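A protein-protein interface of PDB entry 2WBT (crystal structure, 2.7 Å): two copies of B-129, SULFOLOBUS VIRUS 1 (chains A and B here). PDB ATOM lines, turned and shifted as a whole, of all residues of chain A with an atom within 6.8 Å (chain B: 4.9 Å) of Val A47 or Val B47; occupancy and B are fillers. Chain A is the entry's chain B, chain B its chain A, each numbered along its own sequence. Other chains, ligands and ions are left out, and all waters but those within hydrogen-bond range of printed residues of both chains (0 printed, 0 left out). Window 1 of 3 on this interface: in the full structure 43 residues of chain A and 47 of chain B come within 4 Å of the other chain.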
ATOM      1  N   ILE A  20     -27.899 -35.689   0.236  1.00  0.00           N
ATOM      2  CA  ILE A  20     -27.552 -36.020   1.621  1.00  0.00           C
ATOM      3  C   ILE A  20     -28.318 -35.148   2.616  1.00  0.00           C
ATOM      4  O   ILE A  20     -28.635 -33.992   2.330  1.00  0.00           O
ATOM      5  CB  ILE A  20     -26.029 -35.880   1.883  1.00  0.00           C
ATOM      6  CG1 ILE A  20     -25.545 -34.449   1.608  1.00  0.00           C
ATOM      7  CG2 ILE A  20     -25.255 -36.873   1.029  1.00  0.00           C
ATOM      8  CD1 ILE A  20     -24.058 -34.256   1.831  1.00  0.00           C
ATOM      9  N   ILE A  22     -28.145 -33.296   6.177  1.00  0.00           N
ATOM     10  CA  ILE A  22     -27.303 -32.777   7.255  1.00  0.00           C
ATOM     11  C   ILE A  22     -28.188 -32.591   8.489  1.00  0.00           C
ATOM     12  O   ILE A  22     -29.120 -31.784   8.475  1.00  0.00           O
ATOM     13  CB  ILE A  22     -26.623 -31.450   6.863  1.00  0.00           C
ATOM     14  CG1 ILE A  22     -25.896 -31.604   5.521  1.00  0.00           C
ATOM     15  CG2 ILE A  22     -25.655 -31.007   7.954  1.00  0.00           C
ATOM     16  CD1 ILE A  22     -25.011 -30.429   5.163  1.00  0.00           C
ATOM     17  N   VAL A  24     -29.516 -31.216  11.080  1.00  0.00           N
ATOM     18  CA  VAL A  24     -29.680 -29.947  11.788  1.00  0.00           C
ATOM     19  C   VAL A  24     -30.970 -30.000  12.612  1.00  0.00           C
ATOM     20  O   VAL A  24     -31.856 -30.805  12.318  1.00  0.00           O
ATOM     21  CB  VAL A  24     -29.696 -28.761  10.776  1.00  0.00           C
ATOM     22  CG1 VAL A  24     -30.920 -27.880  10.950  1.00  0.00           C
ATOM     23  CG2 VAL A  24     -28.407 -27.951  10.879  1.00  0.00           C
ATOM     24  N   TYR A  32     -32.952 -22.149   8.321  1.00  0.00           N
ATOM     25  CA  TYR A  32     -32.247 -22.376   7.057  1.00  0.00           C
ATOM     26  C   TYR A  32     -33.085 -21.962   5.850  1.00  0.00           C
ATOM     27  O   TYR A  32     -32.612 -21.232   4.980  1.00  0.00           O
ATOM     28  CB  TYR A  32     -31.855 -23.851   6.921  1.00  0.00           C
ATOM     29  CG  TYR A  32     -31.308 -24.214   5.558  1.00  0.00           C
ATOM     30  CD1 TYR A  32     -32.092 -24.897   4.628  1.00  0.00           C
ATOM     31  CD2 TYR A  32     -30.011 -23.867   5.194  1.00  0.00           C
ATOM     32  CE1 TYR A  32     -31.594 -25.228   3.375  1.00  0.00           C
ATOM     33  CE2 TYR A  32     -29.504 -24.194   3.944  1.00  0.00           C
ATOM     34  CZ  TYR A  32     -30.298 -24.875   3.040  1.00  0.00           C
ATOM     35  OH  TYR A  32     -29.801 -25.199   1.799  1.00  0.00           O
ATOM     36  N   LEU A  42     -24.796 -20.898  -1.434  1.00  0.00           N
ATOM     37  CA  LEU A  42     -23.472 -20.683  -0.838  1.00  0.00           C
ATOM     38  C   LEU A  42     -23.174 -21.734   0.229  1.00  0.00           C
ATOM     39  O   LEU A  42     -22.059 -22.251   0.301  1.00  0.00           O
ATOM     40  CB  LEU A  42     -23.357 -19.281  -0.225  1.00  0.00           C
ATOM     41  CG  LEU A  42     -22.917 -18.159  -1.168  1.00  0.00           C
ATOM     42  CD1 LEU A  42     -23.037 -16.817  -0.472  1.00  0.00           C
ATOM     43  CD2 LEU A  42     -21.492 -18.379  -1.656  1.00  0.00           C
ATOM     44  N   ILE A  43     -24.174 -22.042   1.053  1.00  0.00           N
ATOM     45  CA  ILE A  43     -24.034 -23.051   2.106  1.00  0.00           C
ATOM     46  C   ILE A  43     -23.723 -24.434   1.533  1.00  0.00           C
ATOM     47  O   ILE A  43     -22.768 -25.082   1.961  1.00  0.00           O
ATOM     48  CB  ILE A  43     -25.300 -23.139   2.995  1.00  0.00           C
ATOM     49  CG1 ILE A  43     -25.306 -22.008   4.027  1.00  0.00           C
ATOM     50  CG2 ILE A  43     -25.368 -24.485   3.711  1.00  0.00           C
ATOM     51  CD1 ILE A  43     -26.466 -22.072   5.002  1.00  0.00           C
ATOM     52  N   ARG A  44     -24.528 -24.884   0.574  1.00  0.00           N
ATOM     53  CA  ARG A  44     -24.323 -26.210  -0.016  1.00  0.00           C
ATOM     54  C   ARG A  44     -23.126 -26.257  -0.972  1.00  0.00           C
ATOM     55  O   ARG A  44     -22.597 -27.332  -1.242  1.00  0.00           O
ATOM     56  CB  ARG A  44     -25.596 -26.724  -0.696  1.00  0.00           C
ATOM     57  CG  ARG A  44     -25.932 -26.084  -2.028  1.00  0.00           C
ATOM     58  CD  ARG A  44     -27.405 -26.292  -2.348  1.00  0.00           C
ATOM     59  NE  ARG A  44     -27.832 -25.553  -3.538  1.00  0.00           N
ATOM     60  CZ  ARG A  44     -28.844 -24.684  -3.588  1.00  0.00           C
ATOM     61  NH1 ARG A  44     -29.586 -24.417  -2.516  1.00  0.00           N
ATOM     62  NH2 ARG A  44     -29.125 -24.080  -4.738  1.00  0.00           N
ATOM     63  N   ALA A  45     -22.703 -25.098  -1.472  1.00  0.00           N
ATOM     64  CA  ALA A  45     -21.442 -24.999  -2.217  1.00  0.00           C
ATOM     65  C   ALA A  45     -20.247 -25.188  -1.277  1.00  0.00           C
ATOM     66  O   ALA A  45     -19.227 -25.759  -1.666  1.00  0.00           O
ATOM     67  CB  ALA A  45     -21.344 -23.659  -2.929  1.00  0.00           C
ATOM     68  N   ILE A  46     -20.387 -24.704  -0.044  1.00  0.00           N
ATOM     69  CA  ILE A  46     -19.344 -24.833   0.978  1.00  0.00           C
ATOM     70  C   ILE A  46     -19.189 -26.281   1.451  1.00  0.00           C
ATOM     71  O   ILE A  46     -18.068 -26.749   1.648  1.00  0.00           O
ATOM     72  CB  ILE A  46     -19.619 -23.905   2.190  1.00  0.00           C
ATOM     73  CG1 ILE A  46     -19.277 -22.456   1.835  1.00  0.00           C
ATOM     74  CG2 ILE A  46     -18.801 -24.328   3.403  1.00  0.00           C
ATOM     75  CD1 ILE A  46     -19.898 -21.438   2.768  1.00  0.00           C
ATOM     76  N   VAL A  47     -20.307 -26.984   1.619  1.00  0.00           N
ATOM     77  CA  VAL A  47     -20.275 -28.384   2.060  1.00  0.00           C
ATOM     78  C   VAL A  47     -19.741 -29.299   0.952  1.00  0.00           C
ATOM     79  O   VAL A  47     -19.133 -30.332   1.234  1.00  0.00           O
ATOM     80  CB  VAL A  47     -21.664 -28.888   2.536  1.00  0.00           C
ATOM     81  CG1 VAL A  47     -22.252 -27.941   3.579  1.00  0.00           C
ATOM     82  CG2 VAL A  47     -22.618 -29.059   1.360  1.00  0.00           C
ATOM     83  N   LYS A  48     -19.973 -28.909  -0.300  1.00  0.00           N
ATOM     84  CA  LYS A  48     -19.441 -29.634  -1.458  1.00  0.00           C
ATOM     85  C   LYS A  48     -17.925 -29.476  -1.576  1.00  0.00           C
ATOM     86  O   LYS A  48     -17.219 -30.441  -1.870  1.00  0.00           O
ATOM     87  CB  LYS A  48     -20.130 -29.171  -2.744  1.00  0.00           C
ATOM     88  CG  LYS A  48     -21.529 -29.744  -2.912  1.00  0.00           C
ATOM     89  CD  LYS A  48     -22.190 -29.270  -4.193  1.00  0.00           C
ATOM     90  CE  LYS A  48     -23.522 -29.972  -4.412  1.00  0.00           C
ATOM     91  NZ  LYS A  48     -24.063 -29.738  -5.780  1.00  0.00           N
ATOM     92  N   THR A  49     -17.437 -28.256  -1.357  1.00  0.00           N
ATOM     93  CA  THR A  49     -15.998 -27.989  -1.270  1.00  0.00           C
ATOM     94  C   THR A  49     -15.349 -28.892  -0.226  1.00  0.00           C
ATOM     95  O   THR A  49     -14.284 -29.467  -0.455  1.00  0.00           O
ATOM     96  CB  THR A  49     -15.720 -26.527  -0.865  1.00  0.00           C
ATOM     97  OG1 THR A  49     -16.487 -25.640  -1.688  1.00  0.00           O
ATOM     98  CG2 THR A  49     -14.238 -26.201  -1.009  1.00  0.00           C
ATOM     99  N   LEU A  50     -16.013 -29.003   0.922  1.00  0.00           N
ATOM    100  CA  LEU A  50     -15.531 -29.814   2.041  1.00  0.00           C
ATOM    101  C   LEU A  50     -15.585 -31.319   1.757  1.00  0.00           C
ATOM    102  O   LEU A  50     -14.711 -32.059   2.204  1.00  0.00           O
ATOM    103  CB  LEU A  50     -16.328 -29.497   3.312  1.00  0.00           C
ATOM    104  CG  LEU A  50     -16.136 -28.098   3.907  1.00  0.00           C
ATOM    105  CD1 LEU A  50     -17.065 -27.899   5.096  1.00  0.00           C
ATOM    106  CD2 LEU A  50     -14.687 -27.867   4.315  1.00  0.00           C
ATOM    107  N   ILE A  51     -16.608 -31.771   1.034  1.00  0.00           N
ATOM    108  CA  ILE A  51     -16.696 -33.179   0.625  1.00  0.00           C
ATOM    109  C   ILE A  51     -15.530 -33.550  -0.298  1.00  0.00           C
ATOM    110  O   ILE A  51     -14.924 -34.612  -0.151  1.00  0.00           O
ATOM    111  CB  ILE A  51     -18.038 -33.493  -0.079  1.00  0.00           C
ATOM    112  CG1 ILE A  51     -19.161 -33.626   0.951  1.00  0.00           C
ATOM    113  CG2 ILE A  51     -17.945 -34.786  -0.881  1.00  0.00           C
ATOM    114  CD1 ILE A  51     -20.545 -33.695   0.339  1.00  0.00           C
ATOM    115  N   HIS A  52     -15.224 -32.661  -1.239  1.00  0.00           N
ATOM    116  CA  HIS A  52     -14.114 -32.864  -2.178  1.00  0.00           C
ATOM    117  C   HIS A  52     -12.747 -32.668  -1.535  1.00  0.00           C
ATOM    118  O   HIS A  52     -11.771 -33.302  -1.940  1.00  0.00           O
ATOM    119  CB  HIS A  52     -14.247 -31.924  -3.375  1.00  0.00           C
ATOM    120  CG  HIS A  52     -15.284 -32.359  -4.360  1.00  0.00           C
ATOM    121  ND1 HIS A  52     -16.383 -31.590  -4.676  1.00  0.00           N
ATOM    122  CD2 HIS A  52     -15.398 -33.497  -5.083  1.00  0.00           C
ATOM    123  CE1 HIS A  52     -17.123 -32.233  -5.562  1.00  0.00           C
ATOM    124  NE2 HIS A  52     -16.549 -33.392  -5.824  1.00  0.00           N
ATOM    125  N   ILE B  20     -31.624 -30.804   6.828  1.00  0.00           N
ATOM    126  CA  ILE B  20     -31.422 -30.139   5.540  1.00  0.00           C
ATOM    127  C   ILE B  20     -31.026 -31.123   4.442  1.00  0.00           C
ATOM    128  O   ILE B  20     -29.991 -31.781   4.542  1.00  0.00           O
ATOM    129  CB  ILE B  20     -30.316 -29.062   5.642  1.00  0.00           C
ATOM    130  CG1 ILE B  20     -30.794 -27.876   6.480  1.00  0.00           C
ATOM    131  CG2 ILE B  20     -29.910 -28.572   4.257  1.00  0.00           C
ATOM    132  CD1 ILE B  20     -29.689 -26.905   6.841  1.00  0.00           C
ATOM    133  N   ILE B  22     -29.424 -31.566   1.140  1.00  0.00           N
ATOM    134  CA  ILE B  22     -28.540 -30.980   0.136  1.00  0.00           C
ATOM    135  C   ILE B  22     -28.415 -31.943  -1.041  1.00  0.00           C
ATOM    136  O   ILE B  22     -27.835 -33.022  -0.906  1.00  0.00           O
ATOM    137  CB  ILE B  22     -27.143 -30.688   0.713  1.00  0.00           C
ATOM    138  CG1 ILE B  22     -27.231 -29.569   1.756  1.00  0.00           C
ATOM    139  CG2 ILE B  22     -26.172 -30.304  -0.398  1.00  0.00           C
ATOM    140  CD1 ILE B  22     -25.887 -29.107   2.278  1.00  0.00           C
ATOM    141  N   ILE B  43     -18.780 -31.118   9.400  1.00  0.00           N
ATOM    142  CA  ILE B  43     -19.568 -30.536   8.309  1.00  0.00           C
ATOM    143  C   ILE B  43     -20.887 -29.974   8.837  1.00  0.00           C
ATOM    144  O   ILE B  43     -21.326 -28.901   8.424  1.00  0.00           O
ATOM    145  CB  ILE B  43     -19.851 -31.567   7.191  1.00  0.00           C
ATOM    146  CG1 ILE B  43     -18.558 -31.922   6.455  1.00  0.00           C
ATOM    147  CG2 ILE B  43     -20.864 -31.020   6.192  1.00  0.00           C
ATOM    148  CD1 ILE B  43     -18.713 -33.052   5.459  1.00  0.00           C
ATOM    149  N   ARG B  44     -21.506 -30.708   9.756  1.00  0.00           N
ATOM    150  CA  ARG B  44     -22.737 -30.270  10.412  1.00  0.00           C
ATOM    151  C   ARG B  44     -22.492 -29.037  11.282  1.00  0.00           C
ATOM    152  O   ARG B  44     -23.273 -28.086  11.252  1.00  0.00           O
ATOM    153  CB  ARG B  44     -23.296 -31.404  11.265  1.00  0.00           C
ATOM    154  CG  ARG B  44     -24.744 -31.233  11.701  1.00  0.00           C
ATOM    155  CD  ARG B  44     -25.096 -32.146  12.874  1.00  0.00           C
ATOM    156  NE  ARG B  44     -24.413 -33.442  12.828  1.00  0.00           N
ATOM    157  CZ  ARG B  44     -24.665 -34.466  13.638  1.00  0.00           C
ATOM    158  NH1 ARG B  44     -25.603 -34.382  14.577  1.00  0.00           N
ATOM    159  NH2 ARG B  44     -23.973 -35.592  13.501  1.00  0.00           N
ATOM    160  N   ALA B  45     -21.403 -29.063  12.047  1.00  0.00           N
ATOM    161  CA  ALA B  45     -21.032 -27.953  12.934  1.00  0.00           C
ATOM    162  C   ALA B  45     -20.812 -26.648  12.167  1.00  0.00           C
ATOM    163  O   ALA B  45     -21.223 -25.578  12.622  1.00  0.00           O
ATOM    164  CB  ALA B  45     -19.786 -28.309  13.732  1.00  0.00           C
ATOM    165  N   ILE B  46     -20.158 -26.745  11.011  1.00  0.00           N
ATOM    166  CA  ILE B  46     -19.951 -25.591  10.131  1.00  0.00           C
ATOM    167  C   ILE B  46     -21.282 -25.069   9.600  1.00  0.00           C
ATOM    168  O   ILE B  46     -21.546 -23.867   9.647  1.00  0.00           O
ATOM    169  CB  ILE B  46     -19.039 -25.936   8.931  1.00  0.00           C
ATOM    170  CG1 ILE B  46     -17.599 -26.144   9.396  1.00  0.00           C
ATOM    171  CG2 ILE B  46     -19.063 -24.817   7.897  1.00  0.00           C
ATOM    172  CD1 ILE B  46     -16.689 -26.707   8.325  1.00  0.00           C
ATOM    173  N   VAL B  47     -22.112 -25.980   9.097  1.00  0.00           N
ATOM    174  CA  VAL B  47     -23.431 -25.623   8.569  1.00  0.00           C
ATOM    175  C   VAL B  47     -24.295 -24.964   9.646  1.00  0.00           C
ATOM    176  O   VAL B  47     -24.999 -23.993   9.370  1.00  0.00           O
ATOM    177  CB  VAL B  47     -24.164 -26.853   7.986  1.00  0.00           C
ATOM    178  CG1 VAL B  47     -25.597 -26.501   7.604  1.00  0.00           C
ATOM    179  CG2 VAL B  47     -23.412 -27.393   6.780  1.00  0.00           C
ATOM    180  N   LYS B  48     -24.226 -25.484  10.871  1.00  0.00           N
ATOM    181  CA  LYS B  48     -24.943 -24.894  12.005  1.00  0.00           C
ATOM    182  C   LYS B  48     -24.451 -23.475  12.302  1.00  0.00           C
ATOM    183  O   LYS B  48     -25.255 -22.572  12.535  1.00  0.00           O
ATOM    184  CB  LYS B  48     -24.802 -25.769  13.254  1.00  0.00           C
ATOM    185  CG  LYS B  48     -25.661 -27.024  13.231  1.00  0.00           C
ATOM    186  CD  LYS B  48     -25.650 -27.732  14.577  1.00  0.00           C
ATOM    187  CE  LYS B  48     -26.540 -28.965  14.570  1.00  0.00           C
ATOM    188  NZ  LYS B  48     -26.946 -29.367  15.946  1.00  0.00           N
ATOM    189  N   THR B  49     -23.132 -23.290  12.294  1.00  0.00           N
ATOM    190  CA  THR B  49     -22.528 -21.968  12.484  1.00  0.00           C
ATOM    191  C   THR B  49     -22.944 -20.998  11.379  1.00  0.00           C
ATOM    192  O   THR B  49     -23.258 -19.837  11.651  1.00  0.00           O
ATOM    193  CB  THR B  49     -20.988 -22.046  12.510  1.00  0.00           C
ATOM    194  OG1 THR B  49     -20.567 -22.993  13.499  1.00  0.00           O
ATOM    195  CG2 THR B  49     -20.383 -20.683  12.830  1.00  0.00           C
ATOM    196  N   LEU B  50     -22.937 -21.480  10.138  1.00  0.00           N
ATOM    197  CA  LEU B  50     -23.345 -20.670   8.986  1.00  0.00           C
ATOM    198  C   LEU B  50     -24.821 -20.274   9.062  1.00  0.00           C
ATOM    199  O   LEU B  50     -25.190 -19.168   8.663  1.00  0.00           O
ATOM    200  CB  LEU B  50     -23.066 -21.413   7.673  1.00  0.00           C
ATOM    201  CG  LEU B  50     -21.595 -21.568   7.270  1.00  0.00           C
ATOM    202  CD1 LEU B  50     -21.475 -22.414   6.013  1.00  0.00           C
ATOM    203  CD2 LEU B  50     -20.928 -20.214   7.072  1.00  0.00           C
ATOM    204  N   ILE B  51     -25.656 -21.180   9.566  1.00  0.00           N
ATOM    205  CA  ILE B  51     -27.078 -20.895   9.786  1.00  0.00           C
ATOM    206  C   ILE B  51     -27.293 -19.782  10.821  1.00  0.00           C
ATOM    207  O   ILE B  51     -28.149 -18.915  10.632  1.00  0.00           O
ATOM    208  CB  ILE B  51     -27.849 -22.168  10.221  1.00  0.00           C
ATOM    209  CG1 ILE B  51     -28.018 -23.120   9.036  1.00  0.00           C
ATOM    210  CG2 ILE B  51     -29.223 -21.811  10.776  1.00  0.00           C
ATOM    211  CD1 ILE B  51     -28.474 -24.508   9.430  1.00  0.00           C
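The backbone NH (N) of Ile B22 is in hydrogen-bond range of the backbone carbonyl oxygen (O) of Ile A20, 2.8 Å away.
The backbone carbonyl oxygen of Ile A20 lies close to the backbone carbonyl oxygen of Ile B20, at 3.4 Å.
The backbone NH (N) of Ile A22 sits at hydrogen-bond distance from the backbone carbonyl oxygen (O) of Ile B20 (2.9 Å).
Ile A22 touches Ile B22.
Arg B44 touches Ile A22.
Val A24 touches Lys B48.
CD1 of Ile B51 touches CG2 of Val A24 (3.7 Å).
Ile B20 touches Tyr A32 (CD1 to CG, 3.4 Å).
Arg A44 touches Ile B22.
CD1 of Ile A46 touches CD1 of Leu B50, at 3.7 Å.
Val A47 touches Ile B22 (CG2 to CD1, 3.4 Å).
Val A47 touches Val B47.
Leu A50 touches Ile B46 (CD1 to CD1, 3.5 Å).
Of chain B, only Ile B22 and Val B47 come within 4 Å of Val A47.
Of chain A, only Ile A22 and Val A47 come within 4 Å of Val B47.
Printed residues of chain B within 4 Å of Ile A46: Leu B50.
Printed residues of chain B within 4 Å of Leu A50: Ile B46 (3.5 Å).
Of the printed residues of chain B, Ile A20 touches Ile B20 and Ile B22.
Printed residues of chain B within 4 Å of Arg A44: Ile B22 (3.6 Å).
The nearest residue of chain B that does not touch Val A47 is Ile B43 (4.3 Å).
The nearest printed residue of chain A that does not touch Ile B22 is Lys A48 (4.8 Å).
Of the 15 printed residues of chain A, 8 touch a printed residue of chain B.
Ile A20 touches its own counterpart, Ile B20.
Ile B22 touches its own counterpart, Ile A22.
Ile A22 touches Arg B44, and with the chains exchanged Arg A44 touches Ile B22.
Ile A22 touches Val B47, and with the chains exchanged Val A47 touches Ile B22.
Of the 14 pairs that touch across the chains among the printed residues, 11 have their exchanged pair printed and touching as well.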
